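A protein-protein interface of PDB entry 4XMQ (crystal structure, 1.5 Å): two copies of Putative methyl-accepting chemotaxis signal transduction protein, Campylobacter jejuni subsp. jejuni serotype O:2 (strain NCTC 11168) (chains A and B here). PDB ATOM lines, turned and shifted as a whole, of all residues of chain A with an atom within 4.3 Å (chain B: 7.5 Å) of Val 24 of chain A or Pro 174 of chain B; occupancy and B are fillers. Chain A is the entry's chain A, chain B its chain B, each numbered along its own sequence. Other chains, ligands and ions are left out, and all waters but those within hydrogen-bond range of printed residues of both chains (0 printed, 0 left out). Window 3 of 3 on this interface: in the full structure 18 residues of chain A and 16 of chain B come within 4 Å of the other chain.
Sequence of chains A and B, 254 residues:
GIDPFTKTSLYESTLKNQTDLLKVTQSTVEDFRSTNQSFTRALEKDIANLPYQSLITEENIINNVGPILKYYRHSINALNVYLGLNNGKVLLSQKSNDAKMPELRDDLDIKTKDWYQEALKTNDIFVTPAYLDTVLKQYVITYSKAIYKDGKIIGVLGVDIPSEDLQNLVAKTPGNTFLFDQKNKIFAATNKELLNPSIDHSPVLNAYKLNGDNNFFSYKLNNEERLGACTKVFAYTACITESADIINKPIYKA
The backbone carbonyl oxygen (O) of Val 24 of chain A lies within hydrogen-bond range of the side-chain hydroxyl (OG1) of Thr 28 of chain A. The backbone carbonyl oxygen (O) of Val 24 of chain B sits at hydrogen-bond distance from the side-chain hydroxyl (OG1) of Thr 28 of chain B (2.8 Å).
Among the printed residues, pairs that only touch across the chains: Val 24 of chain A with Pro 174 of chain B (3.7 Å), Pro 174 of chain A with Val 24 of chain B (3.7 Å), Asp 20 of chain A with Pro 174 of chain B (3.9 Å) and Leu 21 of chain A with Asp 20 of chain B (3.98 Å).
Val 24 of chain A touches just one residue of chain B: Pro 174 (3.7 Å). Printed residues of chain A within 4 Å of Pro 174 of chain B: Asp 20 (3.9 Å) and Val 24 (3.7 Å). Of the printed residues of chain B, Pro 174 of chain A touches Val 24 (3.7 Å). Printed residues of chain B within 4 Å of Asp 20 of chain A: Pro 174 (3.9 Å). Of the printed residues of chain A, Val 24 of chain B touches Pro 174. Printed residues of chain B within 4 Å of Leu 21 of chain A: Asp 20 (3.98 Å). The nearest residue of chain B that does not touch Val 24 of chain A is Val 24 of chain B (4.1 Å).
Of the 19 printed residues of chain B, 3 touch a printed residue of chain A. Printed residues of chain B that touch a printed residue of chain A: Asp 20, Val 24 and Pro 174. Printed residues of chain A that touch a printed residue of chain B: Asp 20, Leu 21, Val 24 and Pro 174. Hydrophobic or aromatic side chains of chain A within 4 Å of the printed part of chain B: Leu 21, Val 24 and Pro 174. Among the printed residues, no Asp or Glu carboxylate lies within 4 Å of a Lys or Arg side-chain nitrogen of the other chain.
Asp 20 of chain A touches Pro 174 of chain B, but with the chains exchanged Pro 174 of chain A does not touch Asp 20 of chain B (4.4 Å). Leu 21 of chain A touches Asp 20 of chain B, but with the chains exchanged Asp 20 of chain A does not touch Leu 21 of chain B (4.1 Å). Val 24 of chain A touches Pro 174 of chain B, and with the chains exchanged Pro 174 of chain A touches Val 24 of chain B. Of the 4 pairs that touch across the chains among the printed residues, 2 have their exchanged pair printed and touching as well.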
ATOM      1  N   ASP A  20     -31.838  -1.758 -20.366  1.00  0.00           N
ATOM      2  CA  ASP A  20     -30.945  -2.938 -20.339  1.00  0.00           C
ATOM      3  C   ASP A  20     -31.761  -4.225 -20.242  1.00  0.00           C
ATOM      4  O   ASP A  20     -31.461  -5.211 -20.961  1.00  0.00           O
ATOM      5  CB  ASP A  20     -29.983  -2.901 -19.137  1.00  0.00           C
ATOM      6  CG  ASP A  20     -28.791  -1.972 -19.348  1.00  0.00           C
ATOM      7  OD1 ASP A  20     -28.515  -1.539 -20.502  1.00  0.00           O
ATOM      8  OD2 ASP A  20     -28.153  -1.673 -18.293  1.00  0.00           O
ATOM      9  N   LEU A  21     -32.800  -4.235 -19.428  1.00  0.00           N
ATOM     10  CA  LEU A  21     -33.626  -5.428 -19.284  1.00  0.00           C
ATOM     11  C   LEU A  21     -34.406  -5.727 -20.558  1.00  0.00           C
ATOM     12  O   LEU A  21     -34.639  -6.894 -20.905  1.00  0.00           O
ATOM     13  CB  LEU A  21     -34.506  -5.371 -18.045  1.00  0.00           C
ATOM     14  CG  LEU A  21     -33.730  -5.275 -16.713  1.00  0.00           C
ATOM     15  CD1 LEU A  21     -34.700  -5.429 -15.559  1.00  0.00           C
ATOM     16  CD2 LEU A  21     -32.598  -6.293 -16.571  1.00  0.00           C
ATOM     17  N   LEU A  22     -34.891  -4.678 -21.220  1.00  0.00           N
ATOM     18  CA  LEU A  22     -35.597  -4.853 -22.484  1.00  0.00           C
ATOM     19  C   LEU A  22     -34.659  -5.499 -23.506  1.00  0.00           C
ATOM     20  O   LEU A  22     -35.087  -6.391 -24.269  1.00  0.00           O
ATOM     21  CB  LEU A  22     -36.153  -3.530 -22.992  1.00  0.00           C
ATOM     22  CG  LEU A  22     -37.029  -3.567 -24.262  1.00  0.00           C
ATOM     23  CD1 LEU A  22     -38.158  -4.550 -24.117  1.00  0.00           C
ATOM     24  CD2 LEU A  22     -37.528  -2.181 -24.600  1.00  0.00           C
ATOM     25  N   LYS A  23     -33.407  -5.081 -23.538  1.00  0.00           N
ATOM     26  CA  LYS A  23     -32.404  -5.659 -24.435  1.00  0.00           C
ATOM     27  C   LYS A  23     -32.255  -7.156 -24.202  1.00  0.00           C
ATOM     28  O   LYS A  23     -32.142  -7.916 -25.152  1.00  0.00           O
ATOM     29  CB  LYS A  23     -31.038  -4.998 -24.263  1.00  0.00           C
ATOM     30  CG  LYS A  23     -30.907  -3.620 -24.868  1.00  0.00           C
ATOM     31  CD  LYS A  23     -29.437  -3.159 -24.979  1.00  0.00           C
ATOM     32  CE  LYS A  23     -29.381  -1.820 -25.715  1.00  0.00           C
ATOM     33  NZ  LYS A  23     -28.024  -1.425 -26.167  1.00  0.00           N
ATOM     34  N   VAL A  24     -32.312  -7.584 -22.956  1.00  0.00           N
ATOM     35  CA  VAL A  24     -32.183  -9.024 -22.629  1.00  0.00           C
ATOM     36  C   VAL A  24     -33.354  -9.824 -23.223  1.00  0.00           C
ATOM     37  O   VAL A  24     -33.148 -10.902 -23.795  1.00  0.00           O
ATOM     38  CB  VAL A  24     -32.091  -9.273 -21.132  1.00  0.00           C
ATOM     39  CG1 VAL A  24     -32.158 -10.767 -20.817  1.00  0.00           C
ATOM     40  CG2 VAL A  24     -30.828  -8.630 -20.582  1.00  0.00           C
ATOM     41  N   THR A  25     -34.557  -9.299 -23.141  1.00  0.00           N
ATOM     42  CA  THR A  25     -35.723  -9.943 -23.732  1.00  0.00           C
ATOM     43  C   THR A  25     -35.628  -9.921 -25.259  1.00  0.00           C
ATOM     44  O   THR A  25     -35.888 -10.925 -25.907  1.00  0.00           O
ATOM     45  CB  THR A  25     -37.014  -9.312 -23.209  1.00  0.00           C
ATOM     46  OG1 THR A  25     -37.215  -9.731 -21.868  1.00  0.00           O
ATOM     47  CG2 THR A  25     -38.239  -9.727 -24.043  1.00  0.00           C
ATOM     48  N   GLN A  26     -35.191  -8.804 -25.834  1.00  0.00           N
ATOM     49  CA  GLN A  26     -34.940  -8.733 -27.270  1.00  0.00           C
ATOM     50  C   GLN A  26     -33.922  -9.809 -27.701  1.00  0.00           C
ATOM     51  O   GLN A  26     -34.172 -10.579 -28.685  1.00  0.00           O
ATOM     52  CB  GLN A  26     -34.440  -7.356 -27.705  1.00  0.00           C
ATOM     53  CG  GLN A  26     -33.885  -7.332 -29.116  1.00  0.00           C
ATOM     54  CD  GLN A  26     -33.556  -5.936 -29.647  1.00  0.00           C
ATOM     55  OE1 GLN A  26     -33.857  -4.941 -29.035  1.00  0.00           O
ATOM     56  NE2 GLN A  26     -32.843  -5.886 -30.743  1.00  0.00           N
ATOM     57  N   SER A  27     -32.815  -9.918 -26.985  1.00  0.00           N
ATOM     58  CA  SER A  27     -31.799 -10.936 -27.274  1.00  0.00           C
ATOM     59  C   SER A  27     -32.369 -12.348 -27.163  1.00  0.00           C
ATOM     60  O   SER A  27     -32.006 -13.240 -27.943  1.00  0.00           O
ATOM     61  CB  SER A  27     -30.618 -10.758 -26.295  1.00  0.00           C
ATOM     62  OG  SER A  27     -29.906  -9.559 -26.601  1.00  0.00           O
ATOM     63  N   THR A  28     -33.221 -12.578 -26.174  1.00  0.00           N
ATOM     64  CA  THR A  28     -33.848 -13.871 -25.980  1.00  0.00           C
ATOM     65  C   THR A  28     -34.593 -14.278 -27.274  1.00  0.00           C
ATOM     66  O   THR A  28     -34.455 -15.426 -27.755  1.00  0.00           O
ATOM     67  CB  THR A  28     -34.828 -13.849 -24.817  1.00  0.00           C
ATOM     68  OG1 THR A  28     -34.093 -13.546 -23.599  1.00  0.00           O
ATOM     69  CG2 THR A  28     -35.542 -15.148 -24.619  1.00  0.00           C
ATOM     70  N   PRO A 174     -35.204 -11.275 -16.490  1.00  0.00           N
ATOM     71  CA  PRO A 174     -35.442 -10.245 -15.493  1.00  0.00           C
ATOM     72  C   PRO A 174     -36.393  -9.178 -16.037  1.00  0.00           C
ATOM     73  O   PRO A 174     -36.641  -9.094 -17.245  1.00  0.00           O
ATOM     74  CB  PRO A 174     -34.062  -9.642 -15.282  1.00  0.00           C
ATOM     75  CG  PRO A 174     -33.348  -9.888 -16.594  1.00  0.00           C
ATOM     76  CD  PRO A 174     -33.784 -11.264 -16.961  1.00  0.00           C
ATOM     77  N   ASN B  17     -30.052  -3.556 -10.069  1.00  0.00           N
ATOM     78  CA  ASN B  17     -29.763  -3.692 -11.519  1.00  0.00           C
ATOM     79  C   ASN B  17     -28.482  -4.527 -11.695  1.00  0.00           C
ATOM     80  O   ASN B  17     -28.405  -5.384 -12.585  1.00  0.00           O
ATOM     81  CB  ASN B  17     -29.572  -2.321 -12.199  1.00  0.00           C
ATOM     82  CG  ASN B  17     -28.921  -2.391 -13.642  1.00  0.00           C
ATOM     83  OD1 ASN B  17     -29.564  -2.772 -14.623  1.00  0.00           O
ATOM     84  ND2 ASN B  17     -27.638  -1.928 -13.760  1.00  0.00           N
ATOM     85  N   GLN B  18     -27.487  -4.338 -10.828  1.00  0.00           N
ATOM     86  CA  GLN B  18     -26.253  -5.128 -10.944  1.00  0.00           C
ATOM     87  C   GLN B  18     -26.542  -6.589 -10.634  1.00  0.00           C
ATOM     88  O   GLN B  18     -26.027  -7.497 -11.288  1.00  0.00           O
ATOM     89  CB  GLN B  18     -25.132  -4.591 -10.040  1.00  0.00           C
ATOM     90  CG  GLN B  18     -24.640  -3.189 -10.418  1.00  0.00           C
ATOM     91  CD  GLN B  18     -24.024  -3.174 -11.812  1.00  0.00           C
ATOM     92  OE1 GLN B  18     -24.732  -2.881 -12.813  1.00  0.00           O
ATOM     93  NE2 GLN B  18     -22.776  -3.546 -11.905  1.00  0.00           N
ATOM     94  N   ASP B  20     -29.451  -8.113 -11.118  1.00  0.00           N
ATOM     95  CA  ASP B  20     -30.166  -8.600 -12.281  1.00  0.00           C
ATOM     96  C   ASP B  20     -29.231  -8.969 -13.404  1.00  0.00           C
ATOM     97  O   ASP B  20     -29.391 -10.000 -14.059  1.00  0.00           O
ATOM     98  CB  ASP B  20     -31.164  -7.535 -12.760  1.00  0.00           C
ATOM     99  CG  ASP B  20     -32.397  -7.446 -11.868  1.00  0.00           C
ATOM    100  OD1 ASP B  20     -32.683  -8.345 -11.057  1.00  0.00           O
ATOM    101  OD2 ASP B  20     -33.123  -6.485 -12.056  1.00  0.00           O
ATOM    102  N   LEU B  21     -28.253  -8.121 -13.666  1.00  0.00           N
ATOM    103  CA  LEU B  21     -27.304  -8.363 -14.773  1.00  0.00           C
ATOM    104  C   LEU B  21     -26.359  -9.522 -14.494  1.00  0.00           C
ATOM    105  O   LEU B  21     -26.078 -10.335 -15.376  1.00  0.00           O
ATOM    106  CB  LEU B  21     -26.561  -7.112 -15.140  1.00  0.00           C
ATOM    107  CG  LEU B  21     -27.468  -5.978 -15.698  1.00  0.00           C
ATOM    108  CD1 LEU B  21     -26.607  -4.773 -16.062  1.00  0.00           C
ATOM    109  CD2 LEU B  21     -28.282  -6.407 -16.881  1.00  0.00           C
ATOM    110  N   LEU B  22     -25.904  -9.659 -13.251  1.00  0.00           N
ATOM    111  CA  LEU B  22     -25.119 -10.826 -12.890  1.00  0.00           C
ATOM    112  C   LEU B  22     -25.940 -12.085 -13.126  1.00  0.00           C
ATOM    113  O   LEU B  22     -25.414 -13.077 -13.659  1.00  0.00           O
ATOM    114  CB  LEU B  22     -24.626 -10.739 -11.437  1.00  0.00           C
ATOM    115  CG  LEU B  22     -23.832 -11.939 -10.935  1.00  0.00           C
ATOM    116  CD1 LEU B  22     -22.627 -12.163 -11.797  1.00  0.00           C
ATOM    117  CD2 LEU B  22     -23.446 -11.740  -9.472  1.00  0.00           C
ATOM    118  N   VAL B  24     -28.300 -12.540 -15.276  1.00  0.00           N
ATOM    119  CA  VAL B  24     -28.350 -12.817 -16.732  1.00  0.00           C
ATOM    120  C   VAL B  24     -27.164 -13.660 -17.189  1.00  0.00           C
ATOM    121  O   VAL B  24     -27.289 -14.609 -17.993  1.00  0.00           O
ATOM    122  CB  VAL B  24     -28.467 -11.526 -17.584  1.00  0.00           C
ATOM    123  CG1 VAL B  24     -28.261 -11.864 -19.059  1.00  0.00           C
ATOM    124  CG2 VAL B  24     -29.830 -10.859 -17.309  1.00  0.00           C
ATOM    125  N   THR B  25     -25.966 -13.289 -16.732  1.00  0.00           N
ATOM    126  CA  THR B  25     -24.768 -13.979 -17.088  1.00  0.00           C
ATOM    127  C   THR B  25     -24.815 -15.389 -16.508  1.00  0.00           C
ATOM    128  O   THR B  25     -24.416 -16.356 -17.156  1.00  0.00           O
ATOM    129  CB  THR B  25     -23.504 -13.190 -16.739  1.00  0.00           C
ATOM    130  OG1 THR B  25     -23.357 -12.076 -17.654  1.00  0.00           O
ATOM    131  CG2 THR B  25     -22.292 -14.023 -16.758  1.00  0.00           C
ATOM    132  N   THR B  28     -27.015 -17.382 -18.636  1.00  0.00           N
ATOM    133  CA  THR B  28     -26.334 -17.695 -19.907  1.00  0.00           C
ATOM    134  C   THR B  28     -25.544 -18.987 -19.796  1.00  0.00           C
ATOM    135  O   THR B  28     -25.621 -19.858 -20.675  1.00  0.00           O
ATOM    136  CB  THR B  28     -25.418 -16.544 -20.318  1.00  0.00           C
ATOM    137  OG1 THR B  28     -26.208 -15.338 -20.509  1.00  0.00           O
ATOM    138  CG2 THR B  28     -24.653 -16.890 -21.542  1.00  0.00           C
ATOM    139  N   LEU B 169     -21.606 -15.296 -26.169  1.00  0.00           N
ATOM    140  CA  LEU B 169     -22.878 -15.097 -25.521  1.00  0.00           C
ATOM    141  C   LEU B 169     -22.684 -14.269 -24.228  1.00  0.00           C
ATOM    142  O   LEU B 169     -23.452 -13.357 -23.967  1.00  0.00           O
ATOM    143  CB  LEU B 169     -23.520 -16.467 -25.167  1.00  0.00           C
ATOM    144  CG  LEU B 169     -24.371 -17.132 -26.277  1.00  0.00           C
ATOM    145  CD1 LEU B 169     -24.684 -18.554 -25.879  1.00  0.00           C
ATOM    146  CD2 LEU B 169     -25.653 -16.342 -26.556  1.00  0.00           C
ATOM    147  N   VAL B 170     -21.647 -14.612 -23.463  1.00  0.00           N
ATOM    148  CA  VAL B 170     -21.326 -13.812 -22.243  1.00  0.00           C
ATOM    149  C   VAL B 170     -21.014 -12.382 -22.608  1.00  0.00           C
ATOM    150  O   VAL B 170     -21.538 -11.416 -22.011  1.00  0.00           O
ATOM    151  CB  VAL B 170     -20.234 -14.472 -21.450  1.00  0.00           C
ATOM    152  CG1 VAL B 170     -19.689 -13.522 -20.386  1.00  0.00           C
ATOM    153  CG2 VAL B 170     -20.739 -15.782 -20.826  1.00  0.00           C
ATOM    154  N   ALA B 171     -20.191 -12.229 -23.623  1.00  0.00           N
ATOM    155  CA  ALA B 171     -19.782 -10.890 -24.066  1.00  0.00           C
ATOM    156  C   ALA B 171     -20.907 -10.000 -24.405  1.00  0.00           C
ATOM    157  O   ALA B 171     -20.865  -8.809 -24.105  1.00  0.00           O
ATOM    158  CB  ALA B 171     -18.840 -10.989 -25.240  1.00  0.00           C
ATOM    159  N   LYS B 172     -21.956 -10.557 -25.020  1.00  0.00           N
ATOM    160  CA  LYS B 172     -23.107  -9.740 -25.461  1.00  0.00           C
ATOM    161  C   LYS B 172     -24.108  -9.384 -24.345  1.00  0.00           C
ATOM    162  O   LYS B 172     -24.995  -8.551 -24.527  1.00  0.00           O
ATOM    163  CB  LYS B 172     -23.882 -10.484 -26.570  1.00  0.00           C
ATOM    164  CG  LYS B 172     -23.187 -10.576 -27.902  1.00  0.00           C
ATOM    165  CD  LYS B 172     -24.008 -11.408 -28.922  1.00  0.00           C
ATOM    166  CE  LYS B 172     -23.251 -11.519 -30.244  1.00  0.00           C
ATOM    167  NZ  LYS B 172     -23.238 -10.237 -30.984  1.00  0.00           N
ATOM    168  N   THR B 173     -23.970  -9.987 -23.157  1.00  0.00           N
ATOM    169  CA  THR B 173     -24.879  -9.650 -22.051  1.00  0.00           C
ATOM    170  C   THR B 173     -24.652  -8.175 -21.617  1.00  0.00           C
ATOM    171  O   THR B 173     -23.508  -7.660 -21.695  1.00  0.00           O
ATOM    172  CB  THR B 173     -24.663 -10.588 -20.849  1.00  0.00           C
ATOM    173  OG1 THR B 173     -23.310 -10.444 -20.355  1.00  0.00           O
ATOM    174  CG2 THR B 173     -24.901 -12.059 -21.194  1.00  0.00           C
ATOM    175  N   PRO B 174     -25.688  -7.504 -21.143  1.00  0.00           N
ATOM    176  CA  PRO B 174     -25.496  -6.156 -20.565  1.00  0.00           C
ATOM    177  C   PRO B 174     -24.659  -6.250 -19.270  1.00  0.00           C
ATOM    178  O   PRO B 174     -24.493  -7.333 -18.681  1.00  0.00           O
ATOM    179  CB  PRO B 174     -26.914  -5.677 -20.225  1.00  0.00           C
ATOM    180  CG  PRO B 174     -27.812  -6.592 -20.998  1.00  0.00           C
ATOM    181  CD  PRO B 174     -27.094  -7.941 -20.982  1.00  0.00           C
ATOM    182  N   GLY B 175     -24.067  -5.142 -18.906  1.00  0.00           N
ATOM    183  CA  GLY B 175     -23.292  -5.079 -17.681  1.00  0.00           C
ATOM    184  C   GLY B 175     -21.862  -5.539 -17.826  1.00  0.00           C
ATOM    185  O   GLY B 175     -21.476  -6.276 -18.753  1.00  0.00           O
ATOM    186  N   ASN B 176     -21.047  -5.112 -16.884  1.00  0.00           N
ATOM    187  CA  ASN B 176     -19.631  -5.456 -16.915  1.00  0.00           C
ATOM    188  C   ASN B 176     -19.432  -6.801 -16.244  1.00  0.00           C
ATOM    189  O   ASN B 176     -18.841  -6.929 -15.167  1.00  0.00           O
ATOM    190  CB  ASN B 176     -18.800  -4.371 -16.250  1.00  0.00           C
ATOM    191  CG  ASN B 176     -17.311  -4.603 -16.358  1.00  0.00           C
ATOM    192  OD1 ASN B 176     -16.788  -4.950 -17.413  1.00  0.00           O
ATOM    193  ND2 ASN B 176     -16.606  -4.407 -15.246  1.00  0.00           N
ATOM    194  N   THR B 177     -19.924  -7.823 -16.903  1.00  0.00           N
ATOM    195  CA  THR B 177     -19.892  -9.206 -16.415  1.00  0.00           C
ATOM    196  C   THR B 177     -18.749 -10.005 -17.046  1.00  0.00           C
ATOM    197  O   THR B 177     -18.275  -9.713 -18.143  1.00  0.00           O
ATOM    198  CB  THR B 177     -21.201  -9.923 -16.597  1.00  0.00           C
ATOM    199  OG1 THR B 177     -21.508 -10.026 -18.002  1.00  0.00           O
ATOM    200  CG2 THR B 177     -22.321  -9.261 -15.859  1.00  0.00           C
ATOM    201  N   THR B 190     -17.622  -9.257 -21.067  1.00  0.00           N
ATOM    202  CA  THR B 190     -18.226  -8.173 -21.870  1.00  0.00           C
ATOM    203  C   THR B 190     -17.141  -7.200 -22.332  1.00  0.00           C
ATOM    204  O   THR B 190     -17.084  -6.808 -23.517  1.00  0.00           O
ATOM    205  CB  THR B 190     -19.370  -7.489 -21.151  1.00  0.00           C
ATOM    206  OG1 THR B 190     -20.450  -8.424 -20.981  1.00  0.00           O
ATOM    207  CG2 THR B 190     -19.888  -6.291 -21.912  1.00  0.00           C
ATOM    208  N   ILE B 240     -19.726  -9.513 -11.623  1.00  0.00           N
ATOM    209  CA  ILE B 240     -19.956  -8.222 -12.191  1.00  0.00           C
ATOM    210  C   ILE B 240     -19.229  -7.187 -11.348  1.00  0.00           C
ATOM    211  O   ILE B 240     -19.204  -7.313 -10.117  1.00  0.00           O
ATOM    212  CB  ILE B 240     -21.475  -7.910 -12.269  1.00  0.00           C
ATOM    213  CG1 ILE B 240     -21.735  -6.678 -13.136  1.00  0.00           C
ATOM    214  CG2 ILE B 240     -22.092  -7.724 -10.848  1.00  0.00           C
ATOM    215  CD1 ILE B 240     -23.209  -6.516 -13.509  1.00  0.00           C
